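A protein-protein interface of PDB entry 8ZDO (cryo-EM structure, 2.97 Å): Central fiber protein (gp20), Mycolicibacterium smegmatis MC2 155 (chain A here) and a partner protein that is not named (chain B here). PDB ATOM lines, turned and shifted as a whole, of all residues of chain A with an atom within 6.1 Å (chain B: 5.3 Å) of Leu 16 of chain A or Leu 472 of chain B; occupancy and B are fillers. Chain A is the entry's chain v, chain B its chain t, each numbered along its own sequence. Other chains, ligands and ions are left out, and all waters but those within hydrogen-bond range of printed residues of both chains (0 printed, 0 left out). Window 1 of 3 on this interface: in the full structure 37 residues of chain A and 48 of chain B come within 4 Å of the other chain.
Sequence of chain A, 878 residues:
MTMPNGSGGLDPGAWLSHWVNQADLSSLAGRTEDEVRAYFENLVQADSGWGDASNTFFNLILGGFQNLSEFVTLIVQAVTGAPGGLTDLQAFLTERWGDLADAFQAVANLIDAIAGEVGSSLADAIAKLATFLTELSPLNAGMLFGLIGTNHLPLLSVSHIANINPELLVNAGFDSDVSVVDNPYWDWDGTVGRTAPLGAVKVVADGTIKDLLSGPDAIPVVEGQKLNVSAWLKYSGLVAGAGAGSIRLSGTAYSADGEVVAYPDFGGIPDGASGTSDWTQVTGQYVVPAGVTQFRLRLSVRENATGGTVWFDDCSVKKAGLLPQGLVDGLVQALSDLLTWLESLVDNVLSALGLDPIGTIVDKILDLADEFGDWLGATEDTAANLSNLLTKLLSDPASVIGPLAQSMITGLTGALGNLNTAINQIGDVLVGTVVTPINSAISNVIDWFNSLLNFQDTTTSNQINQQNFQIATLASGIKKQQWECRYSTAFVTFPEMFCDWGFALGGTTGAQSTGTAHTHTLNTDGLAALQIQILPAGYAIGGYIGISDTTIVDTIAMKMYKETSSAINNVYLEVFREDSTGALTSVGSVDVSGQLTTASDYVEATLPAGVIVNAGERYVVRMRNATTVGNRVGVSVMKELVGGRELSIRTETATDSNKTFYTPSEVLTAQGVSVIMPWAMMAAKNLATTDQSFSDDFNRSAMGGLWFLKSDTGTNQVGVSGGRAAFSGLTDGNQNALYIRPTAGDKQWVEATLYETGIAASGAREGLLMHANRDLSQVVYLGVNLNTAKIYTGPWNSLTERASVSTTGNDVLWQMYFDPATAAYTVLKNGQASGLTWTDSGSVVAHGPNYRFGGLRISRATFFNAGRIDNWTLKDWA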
ATOM      1  N   GLY A   9     -11.480  15.997 -32.616  1.00  0.00           N
ATOM      2  CA  GLY A   9     -11.765  15.004 -31.598  1.00  0.00           C
ATOM      3  C   GLY A   9     -11.106  15.289 -30.265  1.00  0.00           C
ATOM      4  O   GLY A   9     -11.555  14.766 -29.240  1.00  0.00           O
ATOM      5  N   LEU A  10     -10.054  16.101 -30.257  1.00  0.00           N
ATOM      6  CA  LEU A  10      -9.393  16.481 -29.022  1.00  0.00           C
ATOM      7  C   LEU A  10     -10.213  17.526 -28.275  1.00  0.00           C
ATOM      8  O   LEU A  10     -11.049  18.227 -28.849  1.00  0.00           O
ATOM      9  CB  LEU A  10      -7.992  17.025 -29.304  1.00  0.00           C
ATOM     10  CG  LEU A  10      -6.992  16.082 -29.972  1.00  0.00           C
ATOM     11  CD1 LEU A  10      -5.764  16.851 -30.413  1.00  0.00           C
ATOM     12  CD2 LEU A  10      -6.609  14.950 -29.036  1.00  0.00           C
ATOM     13  N   ASP A  11      -9.959  17.626 -26.971  1.00  0.00           N
ATOM     14  CA  ASP A  11     -10.642  18.597 -26.133  1.00  0.00           C
ATOM     15  C   ASP A  11      -9.705  19.759 -25.847  1.00  0.00           C
ATOM     16  O   ASP A  11      -8.714  19.576 -25.126  1.00  0.00           O
ATOM     17  CB  ASP A  11     -11.107  17.953 -24.831  1.00  0.00           C
ATOM     18  CG  ASP A  11     -11.905  16.687 -25.062  1.00  0.00           C
ATOM     19  OD1 ASP A  11     -11.293  15.647 -25.382  1.00  0.00           O
ATOM     20  OD2 ASP A  11     -13.147  16.731 -24.931  1.00  0.00           O
ATOM     21  N   ALA A  14      -8.915  20.555 -21.981  1.00  0.00           N
ATOM     22  CA  ALA A  14      -8.369  19.554 -21.081  1.00  0.00           C
ATOM     23  C   ALA A  14      -7.164  20.107 -20.323  1.00  0.00           C
ATOM     24  O   ALA A  14      -6.562  21.114 -20.701  1.00  0.00           O
ATOM     25  CB  ALA A  14      -7.974  18.297 -21.852  1.00  0.00           C
ATOM     26  N   TRP A  15      -6.822  19.425 -19.228  1.00  0.00           N
ATOM     27  CA  TRP A  15      -5.746  19.892 -18.362  1.00  0.00           C
ATOM     28  C   TRP A  15      -4.408  19.904 -19.090  1.00  0.00           C
ATOM     29  O   TRP A  15      -3.650  20.877 -18.996  1.00  0.00           O
ATOM     30  CB  TRP A  15      -5.674  19.015 -17.112  1.00  0.00           C
ATOM     31  CG  TRP A  15      -4.716  19.502 -16.071  1.00  0.00           C
ATOM     32  CD1 TRP A  15      -3.653  18.823 -15.563  1.00  0.00           C
ATOM     33  CD2 TRP A  15      -4.740  20.769 -15.404  1.00  0.00           C
ATOM     34  NE1 TRP A  15      -3.007  19.587 -14.625  1.00  0.00           N
ATOM     35  CE2 TRP A  15      -3.656  20.788 -14.508  1.00  0.00           C
ATOM     36  CE3 TRP A  15      -5.572  21.890 -15.478  1.00  0.00           C
ATOM     37  CZ2 TRP A  15      -3.382  21.882 -13.694  1.00  0.00           C
ATOM     38  CZ3 TRP A  15      -5.296  22.975 -14.668  1.00  0.00           C
ATOM     39  CH2 TRP A  15      -4.211  22.963 -13.787  1.00  0.00           C
ATOM     40  N   LEU A  16      -4.104  18.838 -19.827  1.00  0.00           N
ATOM     41  CA  LEU A  16      -2.850  18.717 -20.558  1.00  0.00           C
ATOM     42  C   LEU A  16      -3.051  18.833 -22.066  1.00  0.00           C
ATOM     43  O   LEU A  16      -2.319  18.220 -22.844  1.00  0.00           O
ATOM     44  CB  LEU A  16      -2.161  17.395 -20.222  1.00  0.00           C
ATOM     45  CG  LEU A  16      -1.707  17.179 -18.778  1.00  0.00           C
ATOM     46  CD1 LEU A  16      -1.016  15.835 -18.649  1.00  0.00           C
ATOM     47  CD2 LEU A  16      -0.789  18.302 -18.324  1.00  0.00           C
ATOM     48  N   SER A  17      -4.046  19.613 -22.492  1.00  0.00           N
ATOM     49  CA  SER A  17      -4.304  19.757 -23.919  1.00  0.00           C
ATOM     50  C   SER A  17      -3.207  20.554 -24.610  1.00  0.00           C
ATOM     51  O   SER A  17      -2.973  20.375 -25.809  1.00  0.00           O
ATOM     52  CB  SER A  17      -5.665  20.415 -24.146  1.00  0.00           C
ATOM     53  OG  SER A  17      -5.596  21.815 -23.944  1.00  0.00           O
ATOM     54  N   HIS A  18      -2.525  21.432 -23.874  1.00  0.00           N
ATOM     55  CA  HIS A  18      -1.443  22.218 -24.453  1.00  0.00           C
ATOM     56  C   HIS A  18      -0.217  21.373 -24.765  1.00  0.00           C
ATOM     57  O   HIS A  18       0.636  21.802 -25.546  1.00  0.00           O
ATOM     58  CB  HIS A  18      -1.072  23.356 -23.503  1.00  0.00           C
ATOM     59  CG  HIS A  18       0.030  24.236 -24.007  1.00  0.00           C
ATOM     60  ND1 HIS A  18       1.359  23.894 -23.904  1.00  0.00           N
ATOM     61  CD2 HIS A  18      -0.003  25.444 -24.614  1.00  0.00           C
ATOM     62  CE1 HIS A  18       2.101  24.854 -24.426  1.00  0.00           C
ATOM     63  NE2 HIS A  18       1.299  25.807 -24.864  1.00  0.00           N
ATOM     64  N   TRP A  19      -0.113  20.181 -24.182  1.00  0.00           N
ATOM     65  CA  TRP A  19       1.072  19.346 -24.309  1.00  0.00           C
ATOM     66  C   TRP A  19       0.850  18.135 -25.203  1.00  0.00           C
ATOM     67  O   TRP A  19       1.709  17.250 -25.254  1.00  0.00           O
ATOM     68  CB  TRP A  19       1.541  18.902 -22.924  1.00  0.00           C
ATOM     69  CG  TRP A  19       1.660  20.037 -21.966  1.00  0.00           C
ATOM     70  CD1 TRP A  19       0.769  20.388 -21.000  1.00  0.00           C
ATOM     71  CD2 TRP A  19       2.731  20.984 -21.888  1.00  0.00           C
ATOM     72  NE1 TRP A  19       1.217  21.492 -20.320  1.00  0.00           N
ATOM     73  CE2 TRP A  19       2.422  21.876 -20.845  1.00  0.00           C
ATOM     74  CE3 TRP A  19       3.923  21.159 -22.594  1.00  0.00           C
ATOM     75  CZ2 TRP A  19       3.261  22.928 -20.492  1.00  0.00           C
ATOM     76  CZ3 TRP A  19       4.753  22.204 -22.242  1.00  0.00           C
ATOM     77  CH2 TRP A  19       4.419  23.074 -21.200  1.00  0.00           C
ATOM     78  N   VAL A  20      -0.276  18.068 -25.903  1.00  0.00           N
ATOM     79  CA  VAL A  20      -0.534  16.973 -26.830  1.00  0.00           C
ATOM     80  C   VAL A  20       0.143  17.297 -28.153  1.00  0.00           C
ATOM     81  O   VAL A  20      -0.118  18.342 -28.756  1.00  0.00           O
ATOM     82  CB  VAL A  20      -2.040  16.745 -27.016  1.00  0.00           C
ATOM     83  CG1 VAL A  20      -2.288  15.681 -28.066  1.00  0.00           C
ATOM     84  CG2 VAL A  20      -2.676  16.352 -25.698  1.00  0.00           C
ATOM     85  N   PRO B 171       5.173  16.432 -19.650  1.00  0.00           N
ATOM     86  CA  PRO B 171       4.188  16.458 -18.558  1.00  0.00           C
ATOM     87  C   PRO B 171       4.018  15.104 -17.888  1.00  0.00           C
ATOM     88  O   PRO B 171       4.856  14.224 -18.041  1.00  0.00           O
ATOM     89  CB  PRO B 171       2.906  16.917 -19.263  1.00  0.00           C
ATOM     90  CG  PRO B 171       3.060  16.426 -20.659  1.00  0.00           C
ATOM     91  CD  PRO B 171       4.524  16.555 -20.966  1.00  0.00           C
ATOM     92  N   ARG B 172       2.939  14.912 -17.130  1.00  0.00           N
ATOM     93  CA  ARG B 172       2.755  13.651 -16.423  1.00  0.00           C
ATOM     94  C   ARG B 172       2.628  12.487 -17.397  1.00  0.00           C
ATOM     95  O   ARG B 172       3.199  11.415 -17.173  1.00  0.00           O
ATOM     96  CB  ARG B 172       1.534  13.732 -15.510  1.00  0.00           C
ATOM     97  CG  ARG B 172       1.327  12.493 -14.666  1.00  0.00           C
ATOM     98  CD  ARG B 172       0.373  12.749 -13.518  1.00  0.00           C
ATOM     99  NE  ARG B 172       0.602  11.815 -12.423  1.00  0.00           N
ATOM    100  CZ  ARG B 172       1.455  12.025 -11.433  1.00  0.00           C
ATOM    101  NH1 ARG B 172       2.166  13.137 -11.359  1.00  0.00           N
ATOM    102  NH2 ARG B 172       1.601  11.095 -10.493  1.00  0.00           N
ATOM    103  N   ILE B 173       1.890  12.679 -18.489  1.00  0.00           N
ATOM    104  CA  ILE B 173       1.744  11.657 -19.515  1.00  0.00           C
ATOM    105  C   ILE B 173       2.100  12.261 -20.865  1.00  0.00           C
ATOM    106  O   ILE B 173       1.978  13.470 -21.080  1.00  0.00           O
ATOM    107  CB  ILE B 173       0.320  11.058 -19.551  1.00  0.00           C
ATOM    108  CG1 ILE B 173      -0.662  12.034 -20.192  1.00  0.00           C
ATOM    109  CG2 ILE B 173      -0.151  10.689 -18.155  1.00  0.00           C
ATOM    110  CD1 ILE B 173      -1.945  11.386 -20.623  1.00  0.00           C
ATOM    111  N   PHE B 240      -5.574   9.265 -30.718  1.00  0.00           N
ATOM    112  CA  PHE B 240      -4.847   9.866 -29.610  1.00  0.00           C
ATOM    113  C   PHE B 240      -4.246   8.742 -28.783  1.00  0.00           C
ATOM    114  O   PHE B 240      -4.976   7.886 -28.275  1.00  0.00           O
ATOM    115  CB  PHE B 240      -5.767  10.733 -28.751  1.00  0.00           C
ATOM    116  CG  PHE B 240      -5.126  11.219 -27.489  1.00  0.00           C
ATOM    117  CD1 PHE B 240      -4.238  12.278 -27.515  1.00  0.00           C
ATOM    118  CD2 PHE B 240      -5.403  10.612 -26.278  1.00  0.00           C
ATOM    119  CE1 PHE B 240      -3.646  12.725 -26.358  1.00  0.00           C
ATOM    120  CE2 PHE B 240      -4.812  11.054 -25.119  1.00  0.00           C
ATOM    121  CZ  PHE B 240      -3.933  12.112 -25.158  1.00  0.00           C
ATOM    122  N   ASN B 468      -5.862   8.384 -17.074  1.00  0.00           N
ATOM    123  CA  ASN B 468      -6.194   9.807 -17.021  1.00  0.00           C
ATOM    124  C   ASN B 468      -6.026  10.461 -18.388  1.00  0.00           C
ATOM    125  O   ASN B 468      -5.400  11.512 -18.530  1.00  0.00           O
ATOM    126  CB  ASN B 468      -5.340  10.514 -15.973  1.00  0.00           C
ATOM    127  CG  ASN B 468      -5.366   9.808 -14.633  1.00  0.00           C
ATOM    128  OD1 ASN B 468      -6.429   9.449 -14.128  1.00  0.00           O
ATOM    129  ND2 ASN B 468      -4.195   9.614 -14.045  1.00  0.00           N
ATOM    130  N   SER B 469      -6.595   9.840 -19.423  1.00  0.00           N
ATOM    131  CA  SER B 469      -6.525  10.374 -20.775  1.00  0.00           C
ATOM    132  C   SER B 469      -7.883  10.613 -21.420  1.00  0.00           C
ATOM    133  O   SER B 469      -7.937  11.206 -22.506  1.00  0.00           O
ATOM    134  CB  SER B 469      -5.711   9.433 -21.675  1.00  0.00           C
ATOM    135  OG  SER B 469      -6.363   8.185 -21.818  1.00  0.00           O
ATOM    136  N   TRP B 470      -8.972  10.165 -20.793  1.00  0.00           N
ATOM    137  CA  TRP B 470     -10.295  10.363 -21.373  1.00  0.00           C
ATOM    138  C   TRP B 470     -10.633  11.844 -21.481  1.00  0.00           C
ATOM    139  O   TRP B 470     -11.295  12.273 -22.433  1.00  0.00           O
ATOM    140  CB  TRP B 470     -11.343   9.625 -20.541  1.00  0.00           C
ATOM    141  CG  TRP B 470     -11.445  10.114 -19.137  1.00  0.00           C
ATOM    142  CD1 TRP B 470     -10.669   9.745 -18.080  1.00  0.00           C
ATOM    143  CD2 TRP B 470     -12.382  11.069 -18.632  1.00  0.00           C
ATOM    144  NE1 TRP B 470     -11.065  10.410 -16.947  1.00  0.00           N
ATOM    145  CE2 TRP B 470     -12.115  11.231 -17.261  1.00  0.00           C
ATOM    146  CE3 TRP B 470     -13.420  11.804 -19.207  1.00  0.00           C
ATOM    147  CZ2 TRP B 470     -12.847  12.095 -16.459  1.00  0.00           C
ATOM    148  CZ3 TRP B 470     -14.145  12.659 -18.411  1.00  0.00           C
ATOM    149  CH2 TRP B 470     -13.857  12.800 -17.052  1.00  0.00           C
ATOM    150  N   SER B 471     -10.187  12.643 -20.509  1.00  0.00           N
ATOM    151  CA  SER B 471     -10.397  14.083 -20.590  1.00  0.00           C
ATOM    152  C   SER B 471      -9.637  14.688 -21.760  1.00  0.00           C
ATOM    153  O   SER B 471     -10.070  15.698 -22.325  1.00  0.00           O
ATOM    154  CB  SER B 471      -9.981  14.743 -19.277  1.00  0.00           C
ATOM    155  OG  SER B 471      -8.655  14.395 -18.929  1.00  0.00           O
ATOM    156  N   LEU B 472      -8.505  14.090 -22.135  1.00  0.00           N
ATOM    157  CA  LEU B 472      -7.772  14.569 -23.300  1.00  0.00           C
ATOM    158  C   LEU B 472      -8.468  14.168 -24.593  1.00  0.00           C
ATOM    159  O   LEU B 472      -8.536  14.963 -25.537  1.00  0.00           O
ATOM    160  CB  LEU B 472      -6.340  14.037 -23.272  1.00  0.00           C
ATOM    161  CG  LEU B 472      -5.451  14.639 -22.186  1.00  0.00           C
ATOM    162  CD1 LEU B 472      -4.163  13.857 -22.049  1.00  0.00           C
ATOM    163  CD2 LEU B 472      -5.164  16.092 -22.499  1.00  0.00           C
ATOM    164  N   ALA B 473      -8.983  12.942 -24.662  1.00  0.00           N
ATOM    165  CA  ALA B 473      -9.698  12.457 -25.847  1.00  0.00           C
ATOM    166  C   ALA B 473     -10.979  11.762 -25.396  1.00  0.00           C
ATOM    167  O   ALA B 473     -10.996  10.546 -25.186  1.00  0.00           O
ATOM    168  CB  ALA B 473      -8.815  11.531 -26.672  1.00  0.00           C
ATOM    169  N   ALA B 474     -12.047  12.545 -25.242  1.00  0.00           N
ATOM    170  CA  ALA B 474     -13.344  11.990 -24.865  1.00  0.00           C
ATOM    171  C   ALA B 474     -13.853  10.995 -25.902  1.00  0.00           C
ATOM    172  O   ALA B 474     -14.309   9.900 -25.555  1.00  0.00           O
ATOM    173  CB  ALA B 474     -14.352  13.123 -24.673  1.00  0.00           C
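Among the printed residues, pairs that only touch across the chains: Ala 14 of chain A with Ser 471 of chain B (3.4 Å), Leu 16 of chain A with Leu 472 of chain B (3.5 Å), Asp 11 of chain A with Ala 473 of chain B (3.6 Å), Ala 14 of chain A with Leu 472 of chain B (3.6 Å), Val 20 of chain A with Phe 240 of chain B (3.7 Å), Trp 19 of chain A with Pro 171 of chain B (3.7 Å), Ser 17 of chain A with Leu 472 of chain B (3.7 Å), Leu 10 of chain A with Phe 240 of chain B (3.9 Å) and Leu 10 of chain A with Leu 472 of chain B (3.9 Å).
Along chain A the printed residues that touch a printed residue of chain B span positions 10 to 20.
Of the 11 printed residues of chain B, 6 touch a printed residue of chain A.
Along chain B the printed residues that touch a printed residue of chain A span positions 171 to 474.
Among the printed residues, no Asp or Glu carboxylate lies within 4 Å of a Lys or Arg side-chain nitrogen of the other chain.
Printed residues of chain B within 4 Å of Leu 16 of chain A: Leu 472 (3.5 Å).
Leu 472 of chain B touches five residues of chain A.
Printed residues of chain B within 4 Å of Asp 11 of chain A: Ser 471, Leu 472, Ala 473 and Ala 474.
Printed residues of chain A within 4 Å of Ala 474 of chain B: Asp 11 (3.2 Å).
Of the printed residues of chain B, Ala 14 of chain A touches Ser 471 and Leu 472.
Trp 15 of chain A touches none of the printed residues of chain B.
The nearest residue of chain A that does not touch Leu 472 of chain B is Val 20 of chain A (4.1 Å).
O of Leu 472 of chain B lies within hydrogen-bond range of N of Asp 11 of chain A.
The backbone NH (N) of Ala 474 of chain B lies within hydrogen-bond range of the side-chain carboxylate (OD1) of Asp 11 of chain A, at 3.2 Å.
The side-chain carboxylate (OD1) of Asp 11 of chain A lies close to the backbone carbonyl oxygen (O) of Ser 471 of chain B (3.3 Å).
The side-chain hydroxyl (OG) of Ser 17 of chain A sits at hydrogen-bond distance from the backbone carbonyl oxygen (O) of Ala 14 of chain A (3.5 Å).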
